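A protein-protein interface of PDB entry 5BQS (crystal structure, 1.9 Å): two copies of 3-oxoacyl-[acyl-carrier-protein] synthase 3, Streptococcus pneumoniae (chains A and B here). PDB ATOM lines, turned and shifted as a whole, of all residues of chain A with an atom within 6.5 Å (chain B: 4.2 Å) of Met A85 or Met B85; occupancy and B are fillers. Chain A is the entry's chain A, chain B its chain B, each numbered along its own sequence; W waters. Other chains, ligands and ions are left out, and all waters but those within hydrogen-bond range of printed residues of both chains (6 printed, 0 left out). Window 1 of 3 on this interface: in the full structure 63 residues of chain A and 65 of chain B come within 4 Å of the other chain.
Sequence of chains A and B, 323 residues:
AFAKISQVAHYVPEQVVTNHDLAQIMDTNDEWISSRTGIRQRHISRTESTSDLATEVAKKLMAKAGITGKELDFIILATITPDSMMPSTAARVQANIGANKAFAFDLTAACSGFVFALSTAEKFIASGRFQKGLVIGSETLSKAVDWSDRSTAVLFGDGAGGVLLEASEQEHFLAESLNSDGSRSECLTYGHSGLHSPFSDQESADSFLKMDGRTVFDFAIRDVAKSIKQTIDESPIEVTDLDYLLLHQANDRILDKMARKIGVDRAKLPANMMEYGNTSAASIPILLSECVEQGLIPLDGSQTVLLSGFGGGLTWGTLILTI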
ATOM      1  N   THR A  79     -25.789  18.828 -22.764  1.00  0.00           N
ATOM      2  CA  THR A  79     -25.047  19.932 -22.139  1.00  0.00           C
ATOM      3  C   THR A  79     -23.569  19.840 -22.497  1.00  0.00           C
ATOM      4  O   THR A  79     -23.069  18.756 -22.793  1.00  0.00           O
ATOM      5  CB  THR A  79     -25.236  19.939 -20.577  1.00  0.00           C
ATOM      6  OG1 THR A  79     -24.670  21.142 -20.044  1.00  0.00           O
ATOM      7  CG2 THR A  79     -24.641  18.697 -19.872  1.00  0.00           C
ATOM      8  N   ILE A  80     -22.867  20.967 -22.412  1.00  0.00           N
ATOM      9  CA  ILE A  80     -21.400  21.051 -22.507  1.00  0.00           C
ATOM     10  C   ILE A  80     -20.923  21.647 -21.181  1.00  0.00           C
ATOM     11  O   ILE A  80     -19.737  21.875 -21.004  1.00  0.00           O
ATOM     12  CB  ILE A  80     -20.873  21.835 -23.732  1.00  0.00           C
ATOM     13  CG1 ILE A  80     -21.604  23.196 -23.924  1.00  0.00           C
ATOM     14  CG2 ILE A  80     -20.912  20.961 -24.980  1.00  0.00           C
ATOM     15  CD1 ILE A  80     -20.780  24.265 -24.738  1.00  0.00           C
ATOM     16  N   THR A  81     -21.854  21.895 -20.236  1.00  0.00           N
ATOM     17  CA  THR A  81     -21.533  22.477 -18.925  1.00  0.00           C
ATOM     18  C   THR A  81     -22.115  21.602 -17.805  1.00  0.00           C
ATOM     19  O   THR A  81     -22.797  22.121 -16.938  1.00  0.00           O
ATOM     20  CB  THR A  81     -22.025  23.935 -18.875  1.00  0.00           C
ATOM     21  OG1 THR A  81     -23.405  23.960 -19.231  1.00  0.00           O
ATOM     22  CG2 THR A  81     -21.247  24.857 -19.813  1.00  0.00           C
ATOM     23  N   PRO A  82     -21.877  20.271 -17.783  1.00  0.00           N
ATOM     24  CA  PRO A  82     -22.475  19.444 -16.726  1.00  0.00           C
ATOM     25  C   PRO A  82     -21.985  19.814 -15.334  1.00  0.00           C
ATOM     26  O   PRO A  82     -20.859  20.293 -15.189  1.00  0.00           O
ATOM     27  CB  PRO A  82     -22.012  18.032 -17.100  1.00  0.00           C
ATOM     28  CG  PRO A  82     -20.702  18.248 -17.817  1.00  0.00           C
ATOM     29  CD  PRO A  82     -21.004  19.449 -18.656  1.00  0.00           C
ATOM     30  N   ASP A  83     -22.784  19.518 -14.309  1.00  0.00           N
ATOM     31  CA  ASP A  83     -22.362  19.746 -12.916  1.00  0.00           C
ATOM     32  C   ASP A  83     -21.089  18.967 -12.655  1.00  0.00           C
ATOM     33  O   ASP A  83     -20.206  19.446 -11.942  1.00  0.00           O
ATOM     34  CB  ASP A  83     -23.393  19.191 -11.925  1.00  0.00           C
ATOM     35  CG  ASP A  83     -24.769  19.773 -11.987  1.00  0.00           C
ATOM     36  OD1 ASP A  83     -25.207  20.159 -13.108  1.00  0.00           O
ATOM     37  OD2 ASP A  83     -25.461  19.748 -10.941  1.00  0.00           O
ATOM     38  N   SER A  84     -21.040  17.727 -13.185  1.00  0.00           N
ATOM     39  CA  SER A  84     -19.935  16.796 -13.015  1.00  0.00           C
ATOM     40  C   SER A  84     -19.968  15.810 -14.157  1.00  0.00           C
ATOM     41  O   SER A  84     -20.970  15.703 -14.850  1.00  0.00           O
ATOM     42  CB  SER A  84     -20.078  16.038 -11.687  1.00  0.00           C
ATOM     43  OG  SER A  84     -21.353  15.414 -11.570  1.00  0.00           O
ATOM     44  N   MET A  85     -18.876  15.070 -14.334  1.00  0.00           N
ATOM     45  CA  MET A  85     -18.796  14.017 -15.348  1.00  0.00           C
ATOM     46  C   MET A  85     -19.486  12.796 -14.785  1.00  0.00           C
ATOM     47  O   MET A  85     -20.187  12.076 -15.502  1.00  0.00           O
ATOM     48  CB  MET A  85     -17.342  13.716 -15.729  1.00  0.00           C
ATOM     49  CG  MET A  85     -16.675  14.843 -16.531  1.00  0.00           C
ATOM     50  SD  MET A  85     -17.658  15.519 -17.910  1.00  0.00           S
ATOM     51  CE  MET A  85     -17.978  14.056 -18.876  1.00  0.00           C
ATOM     52  N   MET A  86     -19.293  12.592 -13.488  1.00  0.00           N
ATOM     53  CA  MET A  86     -19.853  11.476 -12.759  1.00  0.00           C
ATOM     54  C   MET A  86     -20.366  11.962 -11.403  1.00  0.00           C
ATOM     55  O   MET A  86     -19.572  12.519 -10.638  1.00  0.00           O
ATOM     56  CB  MET A  86     -18.798  10.387 -12.630  1.00  0.00           C
ATOM     57  CG  MET A  86     -19.356   9.072 -12.164  1.00  0.00           C
ATOM     58  SD  MET A  86     -18.127   7.767 -12.175  1.00  0.00           S
ATOM     59  CE  MET A  86     -16.780   8.530 -11.033  1.00  0.00           C
ATOM     60  N   PRO A  87     -21.688  11.835 -11.094  1.00  0.00           N
ATOM     61  CA  PRO A  87     -22.794  11.295 -11.930  1.00  0.00           C
ATOM     62  C   PRO A  87     -23.087  12.214 -13.110  1.00  0.00           C
ATOM     63  O   PRO A  87     -22.713  13.384 -13.082  1.00  0.00           O
ATOM     64  CB  PRO A  87     -23.992  11.348 -10.976  1.00  0.00           C
ATOM     65  CG  PRO A  87     -23.681  12.493 -10.054  1.00  0.00           C
ATOM     66  CD  PRO A  87     -22.203  12.325  -9.796  1.00  0.00           C
ATOM     67  N   SER A  88     -23.761  11.700 -14.149  1.00  0.00           N
ATOM     68  CA  SER A  88     -24.146  12.537 -15.285  1.00  0.00           C
ATOM     69  C   SER A  88     -25.212  13.541 -14.802  1.00  0.00           C
ATOM     70  O   SER A  88     -25.842  13.328 -13.762  1.00  0.00           O
ATOM     71  CB  SER A  88     -24.733  11.684 -16.405  1.00  0.00           C
ATOM     72  OG  SER A  88     -26.002  11.152 -16.047  1.00  0.00           O
ATOM     73  N   THR A  89     -25.427  14.617 -15.565  1.00  0.00           N
ATOM     74  CA  THR A  89     -26.439  15.630 -15.253  1.00  0.00           C
ATOM     75  C   THR A  89     -27.836  15.008 -15.268  1.00  0.00           C
ATOM     76  O   THR A  89     -28.662  15.341 -14.420  1.00  0.00           O
ATOM     77  CB  THR A  89     -26.297  16.813 -16.244  1.00  0.00           C
ATOM     78  OG1 THR A  89     -24.921  17.139 -16.342  1.00  0.00           O
ATOM     79  CG2 THR A  89     -27.039  18.050 -15.802  1.00  0.00           C
ATOM     80  N   ASP A 106     -26.215  11.771 -20.347  1.00  0.00           N
ATOM     81  CA  ASP A 106     -25.984  13.053 -20.987  1.00  0.00           C
ATOM     82  C   ASP A 106     -25.432  12.786 -22.373  1.00  0.00           C
ATOM     83  O   ASP A 106     -24.747  11.800 -22.580  1.00  0.00           O
ATOM     84  CB  ASP A 106     -24.941  13.899 -20.226  1.00  0.00           C
ATOM     85  CG  ASP A 106     -25.319  14.386 -18.863  1.00  0.00           C
ATOM     86  OD1 ASP A 106     -26.483  14.224 -18.482  1.00  0.00           O
ATOM     87  OD2 ASP A 106     -24.431  14.918 -18.160  1.00  0.00           O
ATOM     88  N   THR A 108     -23.203  14.751 -25.500  1.00  0.00           N
ATOM     89  CA  THR A 108     -22.326  15.912 -25.735  1.00  0.00           C
ATOM     90  C   THR A 108     -22.224  16.179 -27.226  1.00  0.00           C
ATOM     91  O   THR A 108     -21.608  15.385 -27.950  1.00  0.00           O
ATOM     92  CB  THR A 108     -20.907  15.668 -25.141  1.00  0.00           C
ATOM     93  OG1 THR A 108     -21.016  15.062 -23.839  1.00  0.00           O
ATOM     94  CG2 THR A 108     -20.065  16.950 -25.085  1.00  0.00           C
ATOM     95  N   ALA A 109     -22.846  17.278 -27.677  1.00  0.00           N
ATOM     96  CA  ALA A 109     -22.831  17.705 -29.084  1.00  0.00           C
ATOM     97  C   ALA A 109     -23.052  19.212 -29.154  1.00  0.00           C
ATOM     98  O   ALA A 109     -23.627  19.733 -30.105  1.00  0.00           O
ATOM     99  CB  ALA A 109     -23.882  16.958 -29.890  1.00  0.00           C
ATOM    100  N   ALA A 110     -22.572  19.913 -28.121  1.00  0.00           N
ATOM    101  CA  ALA A 110     -22.633  21.381 -27.999  1.00  0.00           C
ATOM    102  C   ALA A 110     -23.980  21.984 -28.391  1.00  0.00           C
ATOM    103  O   ALA A 110     -25.003  21.560 -27.882  1.00  0.00           O
ATOM    104  CB  ALA A 110     -21.496  22.028 -28.762  1.00  0.00           C
ATOM    105  N   TYR A 190     -14.196  24.608 -25.585  1.00  0.00           N
ATOM    106  CA  TYR A 190     -14.466  24.747 -24.164  1.00  0.00           C
ATOM    107  C   TYR A 190     -14.177  23.450 -23.401  1.00  0.00           C
ATOM    108  O   TYR A 190     -14.465  22.363 -23.887  1.00  0.00           O
ATOM    109  CB  TYR A 190     -15.936  25.215 -23.880  1.00  0.00           C
ATOM    110  CG  TYR A 190     -16.279  25.105 -22.415  1.00  0.00           C
ATOM    111  CD1 TYR A 190     -15.584  25.847 -21.459  1.00  0.00           C
ATOM    112  CD2 TYR A 190     -17.221  24.188 -21.967  1.00  0.00           C
ATOM    113  CE1 TYR A 190     -15.764  25.620 -20.100  1.00  0.00           C
ATOM    114  CE2 TYR A 190     -17.456  24.000 -20.605  1.00  0.00           C
ATOM    115  CZ  TYR A 190     -16.738  24.733 -19.676  1.00  0.00           C
ATOM    116  OH  TYR A 190     -16.983  24.587 -18.335  1.00  0.00           O
ATOM    117  N   GLY A 191     -13.643  23.604 -22.190  1.00  0.00           N
ATOM    118  CA  GLY A 191     -13.480  22.539 -21.206  1.00  0.00           C
ATOM    119  C   GLY A 191     -12.318  21.595 -21.342  1.00  0.00           C
ATOM    120  O   GLY A 191     -12.379  20.473 -20.815  1.00  0.00           O
ATOM    121  N   HIS A 192     -11.238  22.035 -21.989  1.00  0.00           N
ATOM    122  CA  HIS A 192     -10.022  21.234 -22.110  1.00  0.00           C
ATOM    123  C   HIS A 192      -9.617  20.684 -20.729  1.00  0.00           C
ATOM    124  O   HIS A 192      -9.617  21.423 -19.737  1.00  0.00           O
ATOM    125  CB  HIS A 192      -8.860  22.039 -22.711  1.00  0.00           C
ATOM    126  CG  HIS A 192      -7.571  21.263 -22.747  1.00  0.00           C
ATOM    127  ND1 HIS A 192      -6.631  21.372 -21.730  1.00  0.00           N
ATOM    128  CD2 HIS A 192      -7.144  20.334 -23.637  1.00  0.00           C
ATOM    129  CE1 HIS A 192      -5.655  20.535 -22.049  1.00  0.00           C
ATOM    130  NE2 HIS A 192      -5.922  19.886 -23.189  1.00  0.00           N
ATOM    131  N   SER A 193      -9.311  19.388 -20.676  1.00  0.00           N
ATOM    132  CA  SER A 193      -8.947  18.684 -19.450  1.00  0.00           C
ATOM    133  C   SER A 193      -7.689  17.880 -19.776  1.00  0.00           C
ATOM    134  O   SER A 193      -7.765  16.848 -20.443  1.00  0.00           O
ATOM    135  CB  SER A 193     -10.110  17.787 -19.025  1.00  0.00           C
ATOM    136  OG  SER A 193      -9.782  16.931 -17.950  1.00  0.00           O
ATOM    137  N   ILE B  80     -15.969   9.595 -19.384  1.00  0.00           N
ATOM    138  CA  ILE B  80     -16.197  10.532 -18.284  1.00  0.00           C
ATOM    139  C   ILE B  80     -14.921  11.385 -18.200  1.00  0.00           C
ATOM    140  O   ILE B  80     -14.815  12.247 -17.352  1.00  0.00           O
ATOM    141  CB  ILE B  80     -16.578   9.898 -16.924  1.00  0.00           C
ATOM    142  CG1 ILE B  80     -15.647   8.709 -16.550  1.00  0.00           C
ATOM    143  CG2 ILE B  80     -18.061   9.535 -16.902  1.00  0.00           C
ATOM    144  CD1 ILE B  80     -15.598   8.402 -15.036  1.00  0.00           C
ATOM    145  N   PRO B  82     -13.398  13.225 -21.118  1.00  0.00           N
ATOM    146  CA  PRO B  82     -13.160  13.750 -22.463  1.00  0.00           C
ATOM    147  C   PRO B  82     -12.000  14.725 -22.525  1.00  0.00           C
ATOM    148  O   PRO B  82     -11.731  15.404 -21.538  1.00  0.00           O
ATOM    149  CB  PRO B  82     -14.477  14.464 -22.772  1.00  0.00           C
ATOM    150  CG  PRO B  82     -14.994  14.914 -21.441  1.00  0.00           C
ATOM    151  CD  PRO B  82     -14.710  13.687 -20.611  1.00  0.00           C
ATOM    152  N   SER B  84     -12.079  17.494 -24.018  1.00  0.00           N
ATOM    153  CA  SER B  84     -12.763  18.772 -23.865  1.00  0.00           C
ATOM    154  C   SER B  84     -14.253  18.527 -23.955  1.00  0.00           C
ATOM    155  O   SER B  84     -14.682  17.457 -24.391  1.00  0.00           O
ATOM    156  CB  SER B  84     -12.343  19.733 -24.981  1.00  0.00           C
ATOM    157  OG  SER B  84     -12.528  19.175 -26.275  1.00  0.00           O
ATOM    158  N   MET B  85     -15.042  19.518 -23.548  1.00  0.00           N
ATOM    159  CA  MET B  85     -16.499  19.432 -23.643  1.00  0.00           C
ATOM    160  C   MET B  85     -16.878  19.783 -25.072  1.00  0.00           C
ATOM    161  O   MET B  85     -17.786  19.201 -25.646  1.00  0.00           O
ATOM    162  CB  MET B  85     -17.181  20.391 -22.643  1.00  0.00           C
ATOM    163  CG  MET B  85     -17.036  19.949 -21.177  1.00  0.00           C
ATOM    164  SD  MET B  85     -17.386  18.191 -20.842  1.00  0.00           S
ATOM    165  CE  MET B  85     -19.057  18.056 -21.463  1.00  0.00           C
ATOM    166  N   MET B  86     -16.153  20.729 -25.638  1.00  0.00           N
ATOM    167  CA  MET B  86     -16.363  21.208 -26.980  1.00  0.00           C
ATOM    168  C   MET B  86     -14.996  21.424 -27.643  1.00  0.00           C
ATOM    169  O   MET B  86     -14.187  22.181 -27.092  1.00  0.00           O
ATOM    170  CB  MET B  86     -17.204  22.488 -26.928  1.00  0.00           C
ATOM    171  CG  MET B  86     -17.689  22.972 -28.259  1.00  0.00           C
ATOM    172  SD  MET B  86     -18.777  24.430 -28.045  1.00  0.00           S
ATOM    173  CE  MET B  86     -17.603  25.635 -27.297  1.00  0.00           C
ATOM    174  N   PRO B  87     -14.667  20.699 -28.758  1.00  0.00           N
ATOM    175  CA  PRO B  87     -15.479  19.676 -29.456  1.00  0.00           C
ATOM    176  C   PRO B  87     -15.627  18.414 -28.607  1.00  0.00           C
ATOM    177  O   PRO B  87     -14.829  18.196 -27.691  1.00  0.00           O
ATOM    178  CB  PRO B  87     -14.614  19.329 -30.674  1.00  0.00           C
ATOM    179  CG  PRO B  87     -13.187  19.575 -30.188  1.00  0.00           C
ATOM    180  CD  PRO B  87     -13.339  20.849 -29.400  1.00  0.00           C
ATOM    181  N   SER B  88     -16.623  17.566 -28.917  1.00  0.00           N
ATOM    182  CA  SER B  88     -16.766  16.297 -28.204  1.00  0.00           C
ATOM    183  C   SER B  88     -15.582  15.387 -28.568  1.00  0.00           C
ATOM    184  O   SER B  88     -14.918  15.620 -29.579  1.00  0.00           O
ATOM    185  CB  SER B  88     -18.070  15.614 -28.595  1.00  0.00           C
ATOM    186  OG  SER B  88     -18.036  15.150 -29.938  1.00  0.00           O
ATOM    187  N   THR B 108     -22.486  10.214 -21.790  1.00  0.00           N
ATOM    188  CA  THR B 108     -21.951  10.219 -20.414  1.00  0.00           C
ATOM    189  C   THR B 108     -22.825   9.350 -19.546  1.00  0.00           C
ATOM    190  O   THR B 108     -23.974   9.717 -19.250  1.00  0.00           O
ATOM    191  CB  THR B 108     -21.881  11.667 -19.847  1.00  0.00           C
ATOM    192  OG1 THR B 108     -21.358  12.549 -20.840  1.00  0.00           O
ATOM    193  CG2 THR B 108     -21.077  11.759 -18.528  1.00  0.00           C
ATOM    194  N   TYR B 190     -16.874  12.413  -9.929  1.00  0.00           N
ATOM    195  CA  TYR B 190     -15.737  12.968 -10.644  1.00  0.00           C
ATOM    196  C   TYR B 190     -16.157  14.152 -11.523  1.00  0.00           C
ATOM    197  O   TYR B 190     -17.215  14.124 -12.140  1.00  0.00           O
ATOM    198  CB  TYR B 190     -15.017  11.906 -11.527  1.00  0.00           C
ATOM    199  CG  TYR B 190     -14.016  12.538 -12.470  1.00  0.00           C
ATOM    200  CD1 TYR B 190     -12.917  13.246 -11.980  1.00  0.00           C
ATOM    201  CD2 TYR B 190     -14.226  12.532 -13.851  1.00  0.00           C
ATOM    202  CE1 TYR B 190     -12.101  13.989 -12.828  1.00  0.00           C
ATOM    203  CE2 TYR B 190     -13.370  13.218 -14.715  1.00  0.00           C
ATOM    204  CZ  TYR B 190     -12.299  13.931 -14.198  1.00  0.00           C
ATOM    205  OH  TYR B 190     -11.418  14.569 -15.038  1.00  0.00           O
ATOM    206  N   GLY B 191     -15.273  15.142 -11.605  1.00  0.00           N
ATOM    207  CA  GLY B 191     -15.364  16.263 -12.528  1.00  0.00           C
ATOM    208  C   GLY B 191     -16.300  17.385 -12.180  1.00  0.00           C
ATOM    209  O   GLY B 191     -16.720  18.108 -13.086  1.00  0.00           O
HETATM  210  O   HOH W   1     -13.138  17.941 -20.342  1.00  0.00           O
HETATM  211  O   HOH W   2     -19.693  19.296 -27.767  1.00  0.00           O
HETATM  212  O   HOH W   3     -21.789  15.094 -19.639  1.00  0.00           O
HETATM  213  O   HOH W   4     -25.688   8.588 -16.716  1.00  0.00           O
HETATM  214  O   HOH W   5     -20.436  16.092 -30.790  1.00  0.00           O
HETATM  215  O   HOH W   6     -12.107  15.252 -17.576  1.00  0.00           O
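Thr A79 touches none of the printed residues of chain B. Of chain B, only Ile B80, Pro B82, Met B85, Thr B108, Tyr B190 and Gly B191 come within 4 Å of Met A85. Of the printed residues of chain B, Ser A88 touches Thr B108. Thr A89 touches none of the printed residues of chain B. Met B85 touches just these residues of chain A: Ile A80, Pro A82, Met A85, Thr A108, Tyr A190 and Gly A191. Of the printed residues of chain A, Thr B108 touches Met A85 (3.2 Å), Ser A88 (3.5 Å), Asp A106 (2.9 Å) and Thr A108 (3.9 Å). Printed residues of chain A within 4 Å of Tyr B190: Ser A84 (3.5 Å), Met A85 (2.9 Å) and Met A86 (2.8 Å). The nearest printed residue of chain B that does not touch Met A85 is Ser B84 (7.3 Å).
N of Met A85 sits at hydrogen-bond distance from O of Tyr B190 (2.9 Å). The backbone carbonyl oxygen of Met A86 is in hydrogen-bond range of the backbone NH of Tyr B190. N of Thr B108 is in hydrogen-bond range of O of Asp A106, 2.9 Å away. N of Met B85 is in hydrogen-bond range of O of Tyr A190 (2.9 Å). The backbone NH (N) of Tyr A190 lies within hydrogen-bond range of the backbone carbonyl oxygen (O) of Met B86 (2.9 Å).
Ile A80 touches Met B85, and with the chains exchanged Met A85 touches Ile B80. Ile A80 touches Met B86, and with the chains exchanged Met A86 touches Ile B80. Pro A82 touches Met B85, and with the chains exchanged Met A85 touches Pro B82. Met A86 touches Tyr B190, and with the chains exchanged Tyr A190 touches Met B86. Positions printed for both chains: 80, 82, 84, 85, 86, 87, 88, 108, 190 and 191.
Among the printed residues, pairs that only touch across the chains: Ile A80 with Met B85 (3.3 Å), Ile A80 with Met B86 (3.9 Å), Pro A82 with Met B85 (3.7 Å), Asp A83 with Gly B191 (3.9 Å), Ser A84 with Tyr B190 (3.5 Å), Ser A84 with Gly B191 (3.5 Å), Met A85 with Ile B80 (3.3 Å), Met A85 with Pro B82 (3.7 Å), Met A85 with Met B85 (3.98 Å), Met A85 with Thr B108 (3.2 Å), Met A85 with Gly B191 (3.9 Å), Met A86 with Ile B80 (3.9 Å), Ser A88 with Thr B108 (3.5 Å), Thr A108 with Met B85 (3.3 Å), Thr A108 with Ser B88 (3.6 Å), Thr A108 with Thr B108 (3.9 Å), Ala A110 with Met B86 (3.7 Å), Tyr A190 with Ser B84 (3.6 Å), Gly A191 with Ser B84 (3.5 Å), Gly A191 with Met B85 (3.9 Å), His A192 with Ser B84 (3.9 Å) and Ser A193 with Pro B82 (3.8 Å).
O of Pro A87 is in hydrogen-bond range of OG of Ser A84. The backbone NH (N) of Thr A89 lies within hydrogen-bond range of the side-chain carboxylate (OD2) of Asp A106 (2.8 Å). The side-chain hydroxyl of Ser B84 lies within hydrogen-bond range of the backbone carbonyl oxygen of Pro B87 (2.9 Å).
Water W4 lies within hydrogen-bond range of the side-chain hydroxyl of Ser A88 (2.7 Å) and the backbone carbonyl oxygen of Thr B108 (3.3 Å). Water W1 bridges the backbone carbonyl oxygen of Gly A191 and the backbone carbonyl oxygen of Pro B82. Water W5 lies within hydrogen-bond range of OG of Ser B88 (2.7 Å) and O of Thr A108 (3.2 Å). Water W6 bridges the side-chain hydroxyl (OH) of Tyr B190 and the side-chain hydroxyl (OG) of Ser A193. Water W3 bridges OG1 of Thr B108 (2.8 Å) and OD2 of Asp A106 (3.0 Å). Water W2 bridges O of Met B85 (2.9 Å) and N of Ala A110 (3.0 Å).
Of the 10 printed residues of chain B, 9 touch a printed residue of chain A. Along chain B the printed residues that touch a printed residue of chain A span positions 80 to 191. Among the printed residues, no Asp or Glu carboxylate lies within 4 Å of a Lys or Arg side-chain nitrogen of the other chain.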
